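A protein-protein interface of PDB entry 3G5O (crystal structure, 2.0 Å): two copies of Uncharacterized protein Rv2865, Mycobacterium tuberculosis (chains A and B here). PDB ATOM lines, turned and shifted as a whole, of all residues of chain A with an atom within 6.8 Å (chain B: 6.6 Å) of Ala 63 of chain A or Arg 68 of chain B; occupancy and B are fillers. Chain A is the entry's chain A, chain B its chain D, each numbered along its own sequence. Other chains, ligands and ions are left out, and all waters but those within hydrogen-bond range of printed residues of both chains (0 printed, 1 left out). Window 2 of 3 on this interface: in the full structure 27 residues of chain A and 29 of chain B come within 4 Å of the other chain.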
ATOM      1  N   THR A  58     -14.747  14.878 -31.008  1.00  0.00           N
ATOM      2  CA  THR A  58     -13.684  13.896 -30.949  1.00  0.00           C
ATOM      3  C   THR A  58     -12.713  14.232 -29.808  1.00  0.00           C
ATOM      4  O   THR A  58     -12.274  13.344 -29.059  1.00  0.00           O
ATOM      5  CB  THR A  58     -12.913  13.829 -32.292  1.00  0.00           C
ATOM      6  OG1 THR A  58     -13.839  13.517 -33.333  1.00  0.00           O
ATOM      7  CG2 THR A  58     -11.835  12.765 -32.241  1.00  0.00           C
ATOM      8  N   LEU A  59     -12.354  15.507 -29.728  1.00  0.00           N
ATOM      9  CA  LEU A  59     -11.515  16.016 -28.633  1.00  0.00           C
ATOM     10  C   LEU A  59     -12.130  15.697 -27.278  1.00  0.00           C
ATOM     11  O   LEU A  59     -11.451  15.167 -26.385  1.00  0.00           O
ATOM     12  CB  LEU A  59     -11.333  17.528 -28.736  1.00  0.00           C
ATOM     13  CG  LEU A  59     -10.372  18.084 -29.779  1.00  0.00           C
ATOM     14  CD1 LEU A  59     -10.709  19.552 -29.828  1.00  0.00           C
ATOM     15  CD2 LEU A  59      -8.911  17.872 -29.359  1.00  0.00           C
ATOM     16  N   TYR A  60     -13.419  15.984 -27.123  1.00  0.00           N
ATOM     17  CA  TYR A  60     -14.067  15.652 -25.865  1.00  0.00           C
ATOM     18  C   TYR A  60     -13.916  14.154 -25.510  1.00  0.00           C
ATOM     19  O   TYR A  60     -13.455  13.796 -24.404  1.00  0.00           O
ATOM     20  CB  TYR A  60     -15.572  16.015 -25.886  1.00  0.00           C
ATOM     21  CG  TYR A  60     -16.211  15.508 -24.601  1.00  0.00           C
ATOM     22  CD1 TYR A  60     -16.154  16.268 -23.427  1.00  0.00           C
ATOM     23  CD2 TYR A  60     -16.825  14.263 -24.553  1.00  0.00           C
ATOM     24  CE1 TYR A  60     -16.699  15.782 -22.219  1.00  0.00           C
ATOM     25  CE2 TYR A  60     -17.375  13.785 -23.379  1.00  0.00           C
ATOM     26  CZ  TYR A  60     -17.298  14.544 -22.214  1.00  0.00           C
ATOM     27  OH  TYR A  60     -17.845  14.045 -21.052  1.00  0.00           O
ATOM     28  N   TRP A  61     -14.351  13.299 -26.437  1.00  0.00           N
ATOM     29  CA  TRP A  61     -14.456  11.865 -26.125  1.00  0.00           C
ATOM     30  C   TRP A  61     -13.114  11.187 -25.886  1.00  0.00           C
ATOM     31  O   TRP A  61     -13.002  10.342 -24.960  1.00  0.00           O
ATOM     32  CB  TRP A  61     -15.268  11.107 -27.163  1.00  0.00           C
ATOM     33  CG  TRP A  61     -16.745  11.303 -26.938  1.00  0.00           C
ATOM     34  CD1 TRP A  61     -17.607  12.049 -27.695  1.00  0.00           C
ATOM     35  CD2 TRP A  61     -17.521  10.735 -25.875  1.00  0.00           C
ATOM     36  NE1 TRP A  61     -18.884  11.965 -27.176  1.00  0.00           N
ATOM     37  CE2 TRP A  61     -18.860  11.175 -26.052  1.00  0.00           C
ATOM     38  CE3 TRP A  61     -17.209   9.923 -24.780  1.00  0.00           C
ATOM     39  CZ2 TRP A  61     -19.896  10.818 -25.178  1.00  0.00           C
ATOM     40  CZ3 TRP A  61     -18.251   9.549 -23.896  1.00  0.00           C
ATOM     41  CH2 TRP A  61     -19.573  10.010 -24.108  1.00  0.00           C
ATOM     42  N   LEU A  62     -12.095  11.584 -26.679  1.00  0.00           N
ATOM     43  CA  LEU A  62     -10.736  11.005 -26.495  1.00  0.00           C
ATOM     44  C   LEU A  62     -10.136  11.313 -25.124  1.00  0.00           C
ATOM     45  O   LEU A  62      -9.248  10.594 -24.667  1.00  0.00           O
ATOM     46  CB  LEU A  62      -9.761  11.483 -27.613  1.00  0.00           C
ATOM     47  CG  LEU A  62     -10.035  10.884 -29.001  1.00  0.00           C
ATOM     48  CD1 LEU A  62      -9.082  11.442 -30.026  1.00  0.00           C
ATOM     49  CD2 LEU A  62      -9.906   9.370 -28.963  1.00  0.00           C
ATOM     50  N   ALA A  63     -10.615  12.394 -24.491  1.00  0.00           N
ATOM     51  CA  ALA A  63     -10.151  12.816 -23.152  1.00  0.00           C
ATOM     52  C   ALA A  63     -10.849  12.112 -21.973  1.00  0.00           C
ATOM     53  O   ALA A  63     -10.499  12.376 -20.807  1.00  0.00           O
ATOM     54  CB  ALA A  63     -10.283  14.356 -22.998  1.00  0.00           C
ATOM     55  N   GLN A  64     -11.843  11.248 -22.260  1.00  0.00           N
ATOM     56  CA  GLN A  64     -12.578  10.596 -21.174  1.00  0.00           C
ATOM     57  C   GLN A  64     -11.889   9.300 -20.668  1.00  0.00           C
ATOM     58  O   GLN A  64     -11.312   8.546 -21.449  1.00  0.00           O
ATOM     59  CB  GLN A  64     -14.034  10.337 -21.573  1.00  0.00           C
ATOM     60  CG  GLN A  64     -14.737  11.604 -22.024  1.00  0.00           C
ATOM     61  CD  GLN A  64     -14.548  12.771 -21.035  1.00  0.00           C
ATOM     62  OE1 GLN A  64     -14.827  12.624 -19.848  1.00  0.00           O
ATOM     63  NE2 GLN A  64     -14.096  13.933 -21.537  1.00  0.00           N
ATOM     64  N   PRO A  65     -11.929   9.061 -19.349  1.00  0.00           N
ATOM     65  CA  PRO A  65     -11.214   7.899 -18.799  1.00  0.00           C
ATOM     66  C   PRO A  65     -11.821   6.594 -19.292  1.00  0.00           C
ATOM     67  O   PRO A  65     -13.067   6.484 -19.357  1.00  0.00           O
ATOM     68  CB  PRO A  65     -11.410   8.011 -17.264  1.00  0.00           C
ATOM     69  CG  PRO A  65     -12.520   8.987 -17.036  1.00  0.00           C
ATOM     70  CD  PRO A  65     -12.678   9.844 -18.329  1.00  0.00           C
ATOM     71  N   ILE A  67     -12.100   5.431 -22.173  1.00  0.00           N
ATOM     72  CA  ILE A  67     -12.910   5.556 -23.413  1.00  0.00           C
ATOM     73  C   ILE A  67     -12.750   4.359 -24.362  1.00  0.00           C
ATOM     74  O   ILE A  67     -13.753   3.791 -24.815  1.00  0.00           O
ATOM     75  CB  ILE A  67     -12.765   6.972 -24.158  1.00  0.00           C
ATOM     76  CG1 ILE A  67     -13.784   7.080 -25.313  1.00  0.00           C
ATOM     77  CG2 ILE A  67     -11.347   7.198 -24.668  1.00  0.00           C
ATOM     78  CD1 ILE A  67     -15.244   6.886 -24.831  1.00  0.00           C
ATOM     79  N   ARG A  68     -11.517   3.933 -24.646  1.00  0.00           N
ATOM     80  CA  ARG A  68     -11.338   2.853 -25.626  1.00  0.00           C
ATOM     81  C   ARG A  68     -11.877   1.488 -25.130  1.00  0.00           C
ATOM     82  O   ARG A  68     -12.483   0.725 -25.918  1.00  0.00           O
ATOM     83  CB  ARG A  68      -9.864   2.735 -26.037  1.00  0.00           C
ATOM     84  CG  ARG A  68      -9.365   3.940 -26.822  1.00  0.00           C
ATOM     85  CD  ARG A  68      -7.816   4.026 -26.742  1.00  0.00           C
ATOM     86  NE  ARG A  68      -7.320   5.207 -27.463  1.00  0.00           N
ATOM     87  CZ  ARG A  68      -7.208   6.409 -26.925  1.00  0.00           C
ATOM     88  NH1 ARG A  68      -7.562   6.596 -25.662  1.00  0.00           N
ATOM     89  NH2 ARG A  68      -6.742   7.422 -27.657  1.00  0.00           N
ATOM     90  N   LEU B  62      -4.133  13.336 -27.316  1.00  0.00           N
ATOM     91  CA  LEU B  62      -5.348  12.623 -26.931  1.00  0.00           C
ATOM     92  C   LEU B  62      -5.443  11.251 -27.598  1.00  0.00           C
ATOM     93  O   LEU B  62      -6.181  10.399 -27.096  1.00  0.00           O
ATOM     94  CB  LEU B  62      -6.605  13.449 -27.232  1.00  0.00           C
ATOM     95  CG  LEU B  62      -6.824  14.650 -26.280  1.00  0.00           C
ATOM     96  CD1 LEU B  62      -8.010  15.508 -26.721  1.00  0.00           C
ATOM     97  CD2 LEU B  62      -7.036  14.161 -24.831  1.00  0.00           C
ATOM     98  N   GLN B  64      -3.021   9.226 -27.427  1.00  0.00           N
ATOM     99  CA  GLN B  64      -2.271   8.368 -26.523  1.00  0.00           C
ATOM    100  C   GLN B  64      -3.177   7.811 -25.407  1.00  0.00           C
ATOM    101  O   GLN B  64      -3.707   8.590 -24.591  1.00  0.00           O
ATOM    102  CB  GLN B  64      -1.039   9.119 -25.944  1.00  0.00           C
ATOM    103  CG  GLN B  64      -0.212   9.941 -27.020  1.00  0.00           C
ATOM    104  CD  GLN B  64       0.109   9.114 -28.265  1.00  0.00           C
ATOM    105  OE1 GLN B  64       0.585   7.980 -28.144  1.00  0.00           O
ATOM    106  NE2 GLN B  64      -0.193   9.652 -29.466  1.00  0.00           N
ATOM    107  N   PRO B  65      -3.371   6.477 -25.361  1.00  0.00           N
ATOM    108  CA  PRO B  65      -4.261   5.870 -24.341  1.00  0.00           C
ATOM    109  C   PRO B  65      -3.765   6.211 -22.932  1.00  0.00           C
ATOM    110  O   PRO B  65      -2.570   6.156 -22.682  1.00  0.00           O
ATOM    111  CB  PRO B  65      -4.169   4.345 -24.620  1.00  0.00           C
ATOM    112  CG  PRO B  65      -3.689   4.254 -26.048  1.00  0.00           C
ATOM    113  CD  PRO B  65      -2.815   5.463 -26.290  1.00  0.00           C
ATOM    114  N   GLY B  66      -4.666   6.639 -22.052  1.00  0.00           N
ATOM    115  CA  GLY B  66      -4.286   6.992 -20.667  1.00  0.00           C
ATOM    116  C   GLY B  66      -3.558   8.341 -20.510  1.00  0.00           C
ATOM    117  O   GLY B  66      -2.833   8.539 -19.529  1.00  0.00           O
ATOM    118  N   ILE B  67      -3.721   9.242 -21.481  1.00  0.00           N
ATOM    119  CA  ILE B  67      -2.993  10.513 -21.464  1.00  0.00           C
ATOM    120  C   ILE B  67      -3.287  11.393 -20.218  1.00  0.00           C
ATOM    121  O   ILE B  67      -2.379  11.888 -19.578  1.00  0.00           O
ATOM    122  CB  ILE B  67      -3.200  11.338 -22.789  1.00  0.00           C
ATOM    123  CG1 ILE B  67      -2.378  12.638 -22.782  1.00  0.00           C
ATOM    124  CG2 ILE B  67      -4.655  11.631 -23.025  1.00  0.00           C
ATOM    125  CD1 ILE B  67      -0.921  12.384 -22.722  1.00  0.00           C
ATOM    126  N   ARG B  68      -4.544  11.585 -19.868  1.00  0.00           N
ATOM    127  CA  ARG B  68      -4.832  12.412 -18.712  1.00  0.00           C
ATOM    128  C   ARG B  68      -4.335  11.766 -17.399  1.00  0.00           C
ATOM    129  O   ARG B  68      -3.859  12.476 -16.483  1.00  0.00           O
ATOM    130  CB  ARG B  68      -6.320  12.783 -18.685  1.00  0.00           C
ATOM    131  CG  ARG B  68      -6.627  13.679 -19.908  1.00  0.00           C
ATOM    132  CD  ARG B  68      -8.034  14.149 -19.894  1.00  0.00           C
ATOM    133  NE  ARG B  68      -8.338  15.069 -18.811  1.00  0.00           N
ATOM    134  CZ  ARG B  68      -9.590  15.274 -18.354  1.00  0.00           C
ATOM    135  NH1 ARG B  68     -10.660  14.594 -18.855  1.00  0.00           N
ATOM    136  NH2 ARG B  68      -9.790  16.148 -17.378  1.00  0.00           N
ATOM    137  N   GLU B  69      -4.397  10.437 -17.316  1.00  0.00           N
ATOM    138  CA  GLU B  69      -3.879   9.746 -16.106  1.00  0.00           C
ATOM    139  C   GLU B  69      -2.357   9.907 -16.013  1.00  0.00           C
ATOM    140  O   GLU B  69      -1.827  10.081 -14.922  1.00  0.00           O
ATOM    141  CB  GLU B  69      -4.295   8.239 -16.049  1.00  0.00           C
ATOM    142  CG  GLU B  69      -5.847   8.071 -16.013  1.00  0.00           C
ATOM    143  CD  GLU B  69      -6.533   8.114 -17.428  1.00  0.00           C
ATOM    144  OE1 GLU B  69      -5.985   8.681 -18.407  1.00  0.00           O
ATOM    145  OE2 GLU B  69      -7.649   7.563 -17.554  1.00  0.00           O
ATOM    146  N   SER B  70      -1.650   9.871 -17.154  1.00  0.00           N
ATOM    147  CA  SER B  70      -0.202  10.010 -17.117  1.00  0.00           C
ATOM    148  C   SER B  70       0.170  11.464 -16.775  1.00  0.00           C
ATOM    149  O   SER B  70       1.149  11.663 -16.101  1.00  0.00           O
ATOM    150  CB  SER B  70       0.474   9.555 -18.432  1.00  0.00           C
ATOM    151  OG  SER B  70       0.273  10.536 -19.395  1.00  0.00           O
ATOM    152  N   ILE B  71      -0.619  12.451 -17.239  1.00  0.00           N
ATOM    153  CA  ILE B  71      -0.458  13.860 -16.833  1.00  0.00           C
ATOM    154  C   ILE B  71      -0.691  14.072 -15.320  1.00  0.00           C
ATOM    155  O   ILE B  71       0.062  14.784 -14.669  1.00  0.00           O
ATOM    156  CB  ILE B  71      -1.334  14.826 -17.707  1.00  0.00           C
ATOM    157  CG1 ILE B  71      -0.814  14.856 -19.163  1.00  0.00           C
ATOM    158  CG2 ILE B  71      -1.367  16.248 -17.146  1.00  0.00           C
ATOM    159  CD1 ILE B  71      -1.943  15.260 -20.144  1.00  0.00           C
ATOM    160  N   ALA B  72      -1.711  13.421 -14.760  1.00  0.00           N
ATOM    161  CA  ALA B  72      -1.933  13.433 -13.285  1.00  0.00           C
ATOM    162  C   ALA B  72      -0.716  12.859 -12.537  1.00  0.00           C
ATOM    163  O   ALA B  72      -0.303  13.370 -11.484  1.00  0.00           O
ATOM    164  CB  ALA B  72      -3.192  12.616 -12.937  1.00  0.00           C
ATOM    165  N   GLU B  73      -0.152  11.781 -13.073  1.00  0.00           N
ATOM    166  CA  GLU B  73       1.040  11.230 -12.457  1.00  0.00           C
ATOM    167  C   GLU B  73       2.235  12.210 -12.572  1.00  0.00           C
ATOM    168  O   GLU B  73       2.974  12.411 -11.613  1.00  0.00           O
ATOM    169  CB  GLU B  73       1.403   9.868 -13.030  1.00  0.00           C
ATOM    170  CG  GLU B  73       2.662   9.328 -12.376  1.00  0.00           C
ATOM    171  CD  GLU B  73       3.073   7.965 -12.867  1.00  0.00           C
ATOM    172  OE1 GLU B  73       2.330   7.384 -13.681  1.00  0.00           O
ATOM    173  OE2 GLU B  73       4.151   7.470 -12.428  1.00  0.00           O
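Ala 63 of chain A touches just these residues of chain B: Leu 62 (3.7 Å) and Arg 68 (3.0 Å).
Of chain A, only Ala 63 comes within 4 Å of Arg 68 of chain B.
Of the printed residues of chain A, Pro 65 of chain B touches Arg 68 (3.6 Å).
Of the printed residues of chain B, Pro 65 of chain A touches Glu 69.
Gly 66 of chain B touches none of the printed residues of chain A.
The nearest residue of chain B that does not touch Ala 63 of chain A is Ile 67 of chain B (5.6 Å).
The nearest printed residue of chain B that does not touch Leu 62 of chain A is Ile 67 of chain B (5.0 Å).
The guanidinium group (NH1) of Arg 68 of chain B sits at hydrogen-bond distance from the backbone carbonyl oxygen (O) of Ala 63 of chain A, 3.0 Å away.
NH2 of Arg 68 of chain A lies within hydrogen-bond range of O of Leu 62 of chain B, at 3.1 Å.
Leu 62 of chain B touches its own counterpart, Leu 62 of chain A.
Arg 68 of chain A touches Leu 62 of chain B, but with the chains exchanged Leu 62 of chain A does not touch Arg 68 of chain B (6.1 Å).
Arg 68 of chain A touches Pro 65 of chain B, but with the chains exchanged Pro 65 of chain A does not touch Arg 68 of chain B (5.2 Å).
Positions printed for both chains: 62, 64, 65, 67 and 68.
Among the printed residues, merely in contact across the chains: Leu 59 of chain A with Leu 62 of chain B, Arg 68 of chain A with Pro 65 of chain B, Ala 63 of chain A with Leu 62 of chain B, Leu 62 of chain A with Leu 62 of chain B and Pro 65 of chain A with Glu 69 of chain B.
Printed residues of chain B that touch a printed residue of chain A: Leu 62, Pro 65, Arg 68 and Glu 69.
Hydrophobic or aromatic side chains of chain B that line the printed part of chain A: Leu 62.
Along chain B the printed residues that touch a printed residue of chain A span positions 62 to 69.
Hydrophobic or aromatic side chains of chain A that line the printed part of chain B: Leu 59, Leu 62, Ala 63 and Pro 65.
Among the printed residues, 7 pairs touch across the chains.
Among the printed residues, no Asp or Glu carboxylate lies within 4 Å of a Lys or Arg side-chain nitrogen of the other chain.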
